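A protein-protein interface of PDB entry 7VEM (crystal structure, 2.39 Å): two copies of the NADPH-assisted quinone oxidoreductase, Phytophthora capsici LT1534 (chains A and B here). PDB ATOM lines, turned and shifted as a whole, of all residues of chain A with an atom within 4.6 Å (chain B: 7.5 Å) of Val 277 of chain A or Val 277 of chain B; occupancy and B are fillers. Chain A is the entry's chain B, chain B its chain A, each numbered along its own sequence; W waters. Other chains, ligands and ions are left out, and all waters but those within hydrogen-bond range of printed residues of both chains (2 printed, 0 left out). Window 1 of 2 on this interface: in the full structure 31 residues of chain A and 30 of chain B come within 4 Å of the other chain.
Ile 247 of chain A touches Pro 278 of chain B, and with the chains exchanged Pro 278 of chain A touches Ile 247 of chain B.
Val 277 of chain B touches its own counterpart, Val 277 of chain A.
Leu 288 of chain A touches its own counterpart, Leu 288 of chain B.
Of the 9 pairs that touch across the chains among the printed residues, 4 have their exchanged pair printed and touching as well.
O of Leu 288 of chain A lies within hydrogen-bond range of N of Leu 288 of chain B (2.6 Å).
Of the 10 printed residues of chain A, 6 touch a printed residue of chain B.
Hydrophobic or aromatic side chains of chain A within 4 Å of the printed part of chain B: Ile 247, Val 277 and Pro 278.
Of the 20 printed residues of chain B, 8 touch a printed residue of chain A.
Hydrophobic or aromatic side chains of chain B within 4 Å of the printed part of chain A: Ala 244, Ile 247, Val 262, Met 274, Val 277 and Pro 278.
Among the printed residues, no Asp or Glu carboxylate lies within 4 Å of a Lys or Arg side-chain nitrogen of the other chain.
The side-chain amide oxygen (OD1) of Asn 276 of chain A is in hydrogen-bond range of the backbone NH (N) of Leu 279 of chain A, at 3.1 Å.
Water W1 lies within hydrogen-bond range of O of Pro 275 of chain B, N of Val 277 of chain B and O of Pro 275 of chain A.
Water W2 lies within hydrogen-bond range of the side-chain amide oxygen of Asn 276 of chain A (2.7 Å) and the backbone NH of Ala 244 of chain B (2.8 Å).
Val 277 of chain A touches just one residue of chain B: Val 277 (3.9 Å).
Of chain A, only Val 277 comes within 4 Å of Val 277 of chain B.
Of the printed residues of chain A, Ile 247 of chain B touches Pro 278.
Of the printed residues of chain B, Ala 281 of chain A touches Gly 290.
Of the printed residues of chain A, Leu 288 of chain B touches Leu 288.
Of the printed residues of chain A, Val 262 of chain B touches Pro 278 (3.5 Å).
Of the printed residues of chain B, Leu 288 of chain A touches Leu 288.
The nearest residue of chain B that does not touch Val 277 of chain A is Pro 278 of chain B (4.2 Å).
The nearest residue of chain A that does not touch Val 277 of chain B is Pro 278 of chain A (4.4 Å).
Pro 278 of chain B touches Ile 247 of chain A.
OD1 of Asn 276 of chain A touches CB of Ala 244 of chain B, at 3.6 Å.
ND2 of Asn 276 of chain A touches CE of Met 274 of chain B (3.8 Å).
Val 277 of chain B touches Val 277 of chain A.
N of Ala 244 of chain B touches CG of Pro 278 of chain A (3.9 Å).
CG of Pro 278 of chain A touches CG1 of Ile 247 of chain B, 3.9 Å away.
O of Pro 278 of chain A touches CG1 of Val 262 of chain B, at 3.5 Å.
Gly 290 of chain B touches Ala 281 of chain A (CA to O, 3.7 Å).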
ATOM      1  N   ILE A 247      15.957 -16.002  32.140  1.00  0.00           N
ATOM      2  CA  ILE A 247      15.902 -15.795  30.691  1.00  0.00           C
ATOM      3  C   ILE A 247      16.441 -16.948  29.882  1.00  0.00           C
ATOM      4  O   ILE A 247      15.960 -17.188  28.765  1.00  0.00           O
ATOM      5  CB  ILE A 247      16.590 -14.479  30.239  1.00  0.00           C
ATOM      6  CG1 ILE A 247      16.086 -14.033  28.853  1.00  0.00           C
ATOM      7  CG2 ILE A 247      18.118 -14.603  30.242  1.00  0.00           C
ATOM      8  CD1 ILE A 247      14.693 -13.442  28.894  1.00  0.00           C
ATOM      9  N   ILE A 251      14.137 -18.553  26.833  1.00  0.00           N
ATOM     10  CA  ILE A 251      14.666 -18.700  25.508  1.00  0.00           C
ATOM     11  C   ILE A 251      14.566 -20.156  25.034  1.00  0.00           C
ATOM     12  O   ILE A 251      14.136 -20.429  23.914  1.00  0.00           O
ATOM     13  CB  ILE A 251      16.138 -18.184  25.424  1.00  0.00           C
ATOM     14  CG1 ILE A 251      16.130 -16.650  25.468  1.00  0.00           C
ATOM     15  CG2 ILE A 251      16.805 -18.668  24.131  1.00  0.00           C
ATOM     16  CD1 ILE A 251      17.481 -15.996  25.629  1.00  0.00           C
ATOM     17  N   PRO A 275      23.564 -15.256  31.678  1.00  0.00           N
ATOM     18  CA  PRO A 275      23.622 -16.011  30.427  1.00  0.00           C
ATOM     19  C   PRO A 275      23.915 -15.123  29.186  1.00  0.00           C
ATOM     20  O   PRO A 275      23.546 -13.956  29.169  1.00  0.00           O
ATOM     21  CB  PRO A 275      22.245 -16.654  30.362  1.00  0.00           C
ATOM     22  CG  PRO A 275      21.350 -15.703  31.061  1.00  0.00           C
ATOM     23  CD  PRO A 275      22.171 -14.997  32.100  1.00  0.00           C
ATOM     24  N   ASN A 276      24.610 -15.684  28.202  1.00  0.00           N
ATOM     25  CA  ASN A 276      24.852 -15.033  26.929  1.00  0.00           C
ATOM     26  C   ASN A 276      23.558 -14.985  26.072  1.00  0.00           C
ATOM     27  O   ASN A 276      23.284 -15.877  25.264  1.00  0.00           O
ATOM     28  CB  ASN A 276      25.987 -15.746  26.173  1.00  0.00           C
ATOM     29  CG  ASN A 276      26.518 -14.914  25.011  1.00  0.00           C
ATOM     30  OD1 ASN A 276      25.759 -14.214  24.351  1.00  0.00           O
ATOM     31  ND2 ASN A 276      27.821 -14.977  24.774  1.00  0.00           N
ATOM     32  N   VAL A 277      22.795 -13.905  26.233  1.00  0.00           N
ATOM     33  CA  VAL A 277      21.524 -13.785  25.574  1.00  0.00           C
ATOM     34  C   VAL A 277      21.664 -13.725  24.036  1.00  0.00           C
ATOM     35  O   VAL A 277      20.934 -14.426  23.359  1.00  0.00           O
ATOM     36  CB  VAL A 277      20.699 -12.624  26.168  1.00  0.00           C
ATOM     37  CG1 VAL A 277      19.461 -12.357  25.323  1.00  0.00           C
ATOM     38  CG2 VAL A 277      20.278 -12.924  27.602  1.00  0.00           C
ATOM     39  N   PRO A 278      22.609 -12.931  23.483  1.00  0.00           N
ATOM     40  CA  PRO A 278      22.640 -12.913  22.007  1.00  0.00           C
ATOM     41  C   PRO A 278      22.951 -14.268  21.400  1.00  0.00           C
ATOM     42  O   PRO A 278      22.352 -14.647  20.390  1.00  0.00           O
ATOM     43  CB  PRO A 278      23.730 -11.883  21.663  1.00  0.00           C
ATOM     44  CG  PRO A 278      23.824 -10.994  22.882  1.00  0.00           C
ATOM     45  CD  PRO A 278      23.383 -11.816  24.073  1.00  0.00           C
ATOM     46  N   LEU A 279      23.851 -15.009  22.033  1.00  0.00           N
ATOM     47  CA  LEU A 279      24.191 -16.346  21.576  1.00  0.00           C
ATOM     48  C   LEU A 279      22.986 -17.291  21.644  1.00  0.00           C
ATOM     49  O   LEU A 279      22.722 -18.015  20.686  1.00  0.00           O
ATOM     50  CB  LEU A 279      25.347 -16.913  22.400  1.00  0.00           C
ATOM     51  CG  LEU A 279      25.844 -18.314  21.964  1.00  0.00           C
ATOM     52  CD1 LEU A 279      26.459 -18.294  20.569  1.00  0.00           C
ATOM     53  CD2 LEU A 279      26.819 -18.872  22.999  1.00  0.00           C
ATOM     54  N   LEU A 280      22.283 -17.272  22.777  1.00  0.00           N
ATOM     55  CA  LEU A 280      21.100 -18.117  22.957  1.00  0.00           C
ATOM     56  C   LEU A 280      19.983 -17.700  21.983  1.00  0.00           C
ATOM     57  O   LEU A 280      19.427 -18.530  21.302  1.00  0.00           O
ATOM     58  CB  LEU A 280      20.600 -18.055  24.405  1.00  0.00           C
ATOM     59  CG  LEU A 280      21.474 -18.716  25.491  1.00  0.00           C
ATOM     60  CD1 LEU A 280      20.904 -18.380  26.860  1.00  0.00           C
ATOM     61  CD2 LEU A 280      21.604 -20.234  25.335  1.00  0.00           C
ATOM     62  N   ALA A 281      19.700 -16.405  21.889  1.00  0.00           N
ATOM     63  CA  ALA A 281      18.723 -15.925  20.913  1.00  0.00           C
ATOM     64  C   ALA A 281      19.044 -16.357  19.475  1.00  0.00           C
ATOM     65  O   ALA A 281      18.155 -16.759  18.736  1.00  0.00           O
ATOM     66  CB  ALA A 281      18.584 -14.401  20.986  1.00  0.00           C
ATOM     67  N   LEU A 288      13.549 -11.098  21.557  1.00  0.00           N
ATOM     68  CA  LEU A 288      13.247 -10.513  22.863  1.00  0.00           C
ATOM     69  C   LEU A 288      12.890  -9.082  22.661  1.00  0.00           C
ATOM     70  O   LEU A 288      13.509  -8.394  21.855  1.00  0.00           O
ATOM     71  CB  LEU A 288      14.430 -10.511  23.783  1.00  0.00           C
ATOM     72  CG  LEU A 288      14.836 -11.818  24.397  1.00  0.00           C
ATOM     73  CD1 LEU A 288      15.777 -12.560  23.459  1.00  0.00           C
ATOM     74  CD2 LEU A 288      15.545 -11.510  25.707  1.00  0.00           C
ATOM     75  N   GLY B 243      27.893  -9.696  19.186  1.00  0.00           N
ATOM     76  CA  GLY B 243      27.294 -10.554  20.167  1.00  0.00           C
ATOM     77  C   GLY B 243      27.458  -9.901  21.514  1.00  0.00           C
ATOM     78  O   GLY B 243      27.408  -8.650  21.604  1.00  0.00           O
ATOM     79  N   ALA B 244      27.676 -10.723  22.552  1.00  0.00           N
ATOM     80  CA  ALA B 244      27.672 -10.235  23.938  1.00  0.00           C
ATOM     81  C   ALA B 244      28.695  -9.157  24.235  1.00  0.00           C
ATOM     82  O   ALA B 244      28.438  -8.218  25.024  1.00  0.00           O
ATOM     83  CB  ALA B 244      27.873 -11.394  24.907  1.00  0.00           C
ATOM     84  N   ILE B 247      26.939  -5.972  22.827  1.00  0.00           N
ATOM     85  CA  ILE B 247      25.508  -5.832  22.893  1.00  0.00           C
ATOM     86  C   ILE B 247      25.096  -4.710  23.797  1.00  0.00           C
ATOM     87  O   ILE B 247      24.080  -4.051  23.515  1.00  0.00           O
ATOM     88  CB  ILE B 247      24.815  -7.131  23.317  1.00  0.00           C
ATOM     89  CG1 ILE B 247      23.322  -7.140  22.910  1.00  0.00           C
ATOM     90  CG2 ILE B 247      25.008  -7.388  24.803  1.00  0.00           C
ATOM     91  CD1 ILE B 247      23.051  -7.143  21.411  1.00  0.00           C
ATOM     92  N   GLU B 248      25.867  -4.451  24.853  1.00  0.00           N
ATOM     93  CA  GLU B 248      25.549  -3.297  25.731  1.00  0.00           C
ATOM     94  C   GLU B 248      25.605  -1.963  24.974  1.00  0.00           C
ATOM     95  O   GLU B 248      24.665  -1.190  25.036  1.00  0.00           O
ATOM     96  CB  GLU B 248      26.439  -3.251  26.992  1.00  0.00           C
ATOM     97  CG  GLU B 248      26.237  -2.005  27.885  1.00  0.00           C
ATOM     98  CD  GLU B 248      26.633  -2.185  29.373  1.00  0.00           C
ATOM     99  OE1 GLU B 248      26.228  -1.338  30.204  1.00  0.00           O
ATOM    100  OE2 GLU B 248      27.315  -3.162  29.747  1.00  0.00           O
ATOM    101  N   ILE B 251      22.732  -1.813  22.421  1.00  0.00           N
ATOM    102  CA  ILE B 251      21.429  -1.541  23.033  1.00  0.00           C
ATOM    103  C   ILE B 251      21.259  -0.051  23.287  1.00  0.00           C
ATOM    104  O   ILE B 251      20.234   0.530  22.969  1.00  0.00           O
ATOM    105  CB  ILE B 251      21.165  -2.375  24.325  1.00  0.00           C
ATOM    106  CG1 ILE B 251      20.740  -3.779  23.956  1.00  0.00           C
ATOM    107  CG2 ILE B 251      20.047  -1.762  25.150  1.00  0.00           C
ATOM    108  CD1 ILE B 251      20.785  -4.740  25.141  1.00  0.00           C
ATOM    109  N   VAL B 262      20.375  -9.657  15.785  1.00  0.00           N
ATOM    110  CA  VAL B 262      21.513 -10.447  16.239  1.00  0.00           C
ATOM    111  C   VAL B 262      21.821 -11.507  15.202  1.00  0.00           C
ATOM    112  O   VAL B 262      20.979 -12.386  14.899  1.00  0.00           O
ATOM    113  CB  VAL B 262      21.250 -11.104  17.619  1.00  0.00           C
ATOM    114  CG1 VAL B 262      22.385 -12.061  17.987  1.00  0.00           C
ATOM    115  CG2 VAL B 262      21.092 -10.022  18.699  1.00  0.00           C
ATOM    116  N   MET B 274      29.667  -9.721  31.412  1.00  0.00           N
ATOM    117  CA  MET B 274      28.475 -10.140  30.688  1.00  0.00           C
ATOM    118  C   MET B 274      27.333  -9.233  31.083  1.00  0.00           C
ATOM    119  O   MET B 274      26.950  -9.215  32.262  1.00  0.00           O
ATOM    120  CB  MET B 274      28.115 -11.585  31.046  1.00  0.00           C
ATOM    121  CG  MET B 274      26.979 -12.184  30.244  1.00  0.00           C
ATOM    122  SD  MET B 274      27.366 -12.276  28.501  1.00  0.00           S
ATOM    123  CE  MET B 274      28.429 -13.710  28.293  1.00  0.00           C
ATOM    124  N   PRO B 275      26.773  -8.483  30.117  1.00  0.00           N
ATOM    125  CA  PRO B 275      25.744  -7.528  30.519  1.00  0.00           C
ATOM    126  C   PRO B 275      24.369  -8.183  30.817  1.00  0.00           C
ATOM    127  O   PRO B 275      24.039  -9.298  30.326  1.00  0.00           O
ATOM    128  CB  PRO B 275      25.691  -6.553  29.349  1.00  0.00           C
ATOM    129  CG  PRO B 275      26.224  -7.312  28.187  1.00  0.00           C
ATOM    130  CD  PRO B 275      26.870  -8.589  28.657  1.00  0.00           C
ATOM    131  N   ASN B 276      23.599  -7.492  31.654  1.00  0.00           N
ATOM    132  CA  ASN B 276      22.202  -7.873  31.923  1.00  0.00           C
ATOM    133  C   ASN B 276      21.266  -7.413  30.764  1.00  0.00           C
ATOM    134  O   ASN B 276      20.720  -6.300  30.813  1.00  0.00           O
ATOM    135  CB  ASN B 276      21.730  -7.294  33.277  1.00  0.00           C
ATOM    136  CG  ASN B 276      20.369  -7.827  33.690  1.00  0.00           C
ATOM    137  OD1 ASN B 276      19.612  -8.343  32.867  1.00  0.00           O
ATOM    138  ND2 ASN B 276      20.046  -7.692  34.970  1.00  0.00           N
ATOM    139  N   VAL B 277      21.044  -8.286  29.779  1.00  0.00           N
ATOM    140  CA  VAL B 277      20.309  -7.907  28.541  1.00  0.00           C
ATOM    141  C   VAL B 277      18.798  -7.696  28.717  1.00  0.00           C
ATOM    142  O   VAL B 277      18.249  -6.669  28.250  1.00  0.00           O
ATOM    143  CB  VAL B 277      20.587  -8.896  27.383  1.00  0.00           C
ATOM    144  CG1 VAL B 277      19.665  -8.587  26.172  1.00  0.00           C
ATOM    145  CG2 VAL B 277      22.071  -8.850  26.989  1.00  0.00           C
ATOM    146  N   PRO B 278      18.110  -8.619  29.423  1.00  0.00           N
ATOM    147  CA  PRO B 278      16.717  -8.335  29.755  1.00  0.00           C
ATOM    148  C   PRO B 278      16.520  -6.972  30.402  1.00  0.00           C
ATOM    149  O   PRO B 278      15.617  -6.226  30.015  1.00  0.00           O
ATOM    150  CB  PRO B 278      16.379  -9.459  30.739  1.00  0.00           C
ATOM    151  CG  PRO B 278      17.212 -10.596  30.285  1.00  0.00           C
ATOM    152  CD  PRO B 278      18.521  -9.937  29.934  1.00  0.00           C
ATOM    153  N   LEU B 279      17.391  -6.618  31.353  1.00  0.00           N
ATOM    154  CA  LEU B 279      17.213  -5.340  32.034  1.00  0.00           C
ATOM    155  C   LEU B 279      17.506  -4.127  31.111  1.00  0.00           C
ATOM    156  O   LEU B 279      16.739  -3.123  31.136  1.00  0.00           O
ATOM    157  CB  LEU B 279      18.068  -5.277  33.293  1.00  0.00           C
ATOM    158  CG  LEU B 279      17.909  -4.016  34.163  1.00  0.00           C
ATOM    159  CD1 LEU B 279      16.468  -3.673  34.493  1.00  0.00           C
ATOM    160  CD2 LEU B 279      18.689  -4.238  35.456  1.00  0.00           C
ATOM    161  N   LEU B 280      18.587  -4.228  30.314  1.00  0.00           N
ATOM    162  CA  LEU B 280      18.968  -3.146  29.408  1.00  0.00           C
ATOM    163  C   LEU B 280      17.925  -2.887  28.317  1.00  0.00           C
ATOM    164  O   LEU B 280      17.596  -1.727  28.011  1.00  0.00           O
ATOM    165  CB  LEU B 280      20.326  -3.446  28.752  1.00  0.00           C
ATOM    166  CG  LEU B 280      21.530  -3.303  29.667  1.00  0.00           C
ATOM    167  CD1 LEU B 280      22.705  -4.016  29.041  1.00  0.00           C
ATOM    168  CD2 LEU B 280      21.841  -1.836  29.946  1.00  0.00           C
ATOM    169  N   ALA B 281      17.427  -3.976  27.738  1.00  0.00           N
ATOM    170  CA  ALA B 281      16.382  -3.918  26.747  1.00  0.00           C
ATOM    171  C   ALA B 281      15.064  -3.408  27.325  1.00  0.00           C
ATOM    172  O   ALA B 281      14.355  -2.636  26.655  1.00  0.00           O
ATOM    173  CB  ALA B 281      16.184  -5.288  26.082  1.00  0.00           C
ATOM    174  N   LEU B 282      14.738  -3.830  28.552  1.00  0.00           N
ATOM    175  CA  LEU B 282      13.563  -3.284  29.271  1.00  0.00           C
ATOM    176  C   LEU B 282      13.626  -1.751  29.442  1.00  0.00           C
ATOM    177  O   LEU B 282      12.635  -1.027  29.196  1.00  0.00           O
ATOM    178  CB  LEU B 282      13.412  -3.961  30.627  1.00  0.00           C
ATOM    179  CG  LEU B 282      12.155  -3.563  31.427  1.00  0.00           C
ATOM    180  CD1 LEU B 282      10.845  -3.513  30.636  1.00  0.00           C
ATOM    181  CD2 LEU B 282      11.990  -4.498  32.598  1.00  0.00           C
ATOM    182  N   ILE B 283      14.807  -1.275  29.819  1.00  0.00           N
ATOM    183  CA  ILE B 283      15.078   0.143  29.989  1.00  0.00           C
ATOM    184  C   ILE B 283      15.096   0.889  28.667  1.00  0.00           C
ATOM    185  O   ILE B 283      14.496   1.984  28.591  1.00  0.00           O
ATOM    186  CB  ILE B 283      16.396   0.369  30.786  1.00  0.00           C
ATOM    187  CG1 ILE B 283      16.161   0.015  32.273  1.00  0.00           C
ATOM    188  CG2 ILE B 283      16.941   1.806  30.629  1.00  0.00           C
ATOM    189  CD1 ILE B 283      17.436  -0.396  32.996  1.00  0.00           C
ATOM    190  N   GLN B 284      15.730   0.321  27.632  1.00  0.00           N
ATOM    191  CA  GLN B 284      15.687   0.968  26.320  1.00  0.00           C
ATOM    192  C   GLN B 284      14.372   0.870  25.623  1.00  0.00           C
ATOM    193  O   GLN B 284      14.087   1.744  24.795  1.00  0.00           O
ATOM    194  CB  GLN B 284      16.735   0.463  25.345  1.00  0.00           C
ATOM    195  CG  GLN B 284      18.114   0.932  25.689  1.00  0.00           C
ATOM    196  CD  GLN B 284      18.365   2.352  25.351  1.00  0.00           C
ATOM    197  OE1 GLN B 284      18.100   2.782  24.247  1.00  0.00           O
ATOM    198  NE2 GLN B 284      18.944   3.082  26.289  1.00  0.00           N
ATOM    199  N   CYS B 286      13.525  -1.664  23.493  1.00  0.00           N
ATOM    200  CA  CYS B 286      13.873  -2.072  22.127  1.00  0.00           C
ATOM    201  C   CYS B 286      13.896  -3.552  22.075  1.00  0.00           C
ATOM    202  O   CYS B 286      13.829  -4.211  23.103  1.00  0.00           O
ATOM    203  CB  CYS B 286      15.213  -1.484  21.710  1.00  0.00           C
ATOM    204  SG  CYS B 286      16.622  -2.206  22.528  1.00  0.00           S
ATOM    205  N   LEU B 288      15.414  -7.387  20.432  1.00  0.00           N
ATOM    206  CA  LEU B 288      16.526  -8.153  19.876  1.00  0.00           C
ATOM    207  C   LEU B 288      15.934  -9.327  19.162  1.00  0.00           C
ATOM    208  O   LEU B 288      14.972  -9.898  19.650  1.00  0.00           O
ATOM    209  CB  LEU B 288      17.448  -8.717  20.934  1.00  0.00           C
ATOM    210  CG  LEU B 288      18.437  -7.761  21.574  1.00  0.00           C
ATOM    211  CD1 LEU B 288      17.706  -6.816  22.535  1.00  0.00           C
ATOM    212  CD2 LEU B 288      19.507  -8.537  22.313  1.00  0.00           C
ATOM    213  N   GLY B 290      17.213 -12.985  17.022  1.00  0.00           N
ATOM    214  CA  GLY B 290      18.192 -13.903  16.434  1.00  0.00           C
ATOM    215  C   GLY B 290      17.796 -14.202  14.995  1.00  0.00           C
ATOM    216  O   GLY B 290      16.798 -14.883  14.735  1.00  0.00           O
HETATM  217  O   HOH W   1      22.107 -11.101  29.954  1.00  0.00           O
HETATM  218  O   HOH W   2      26.974 -13.415  22.043  1.00  0.00           O
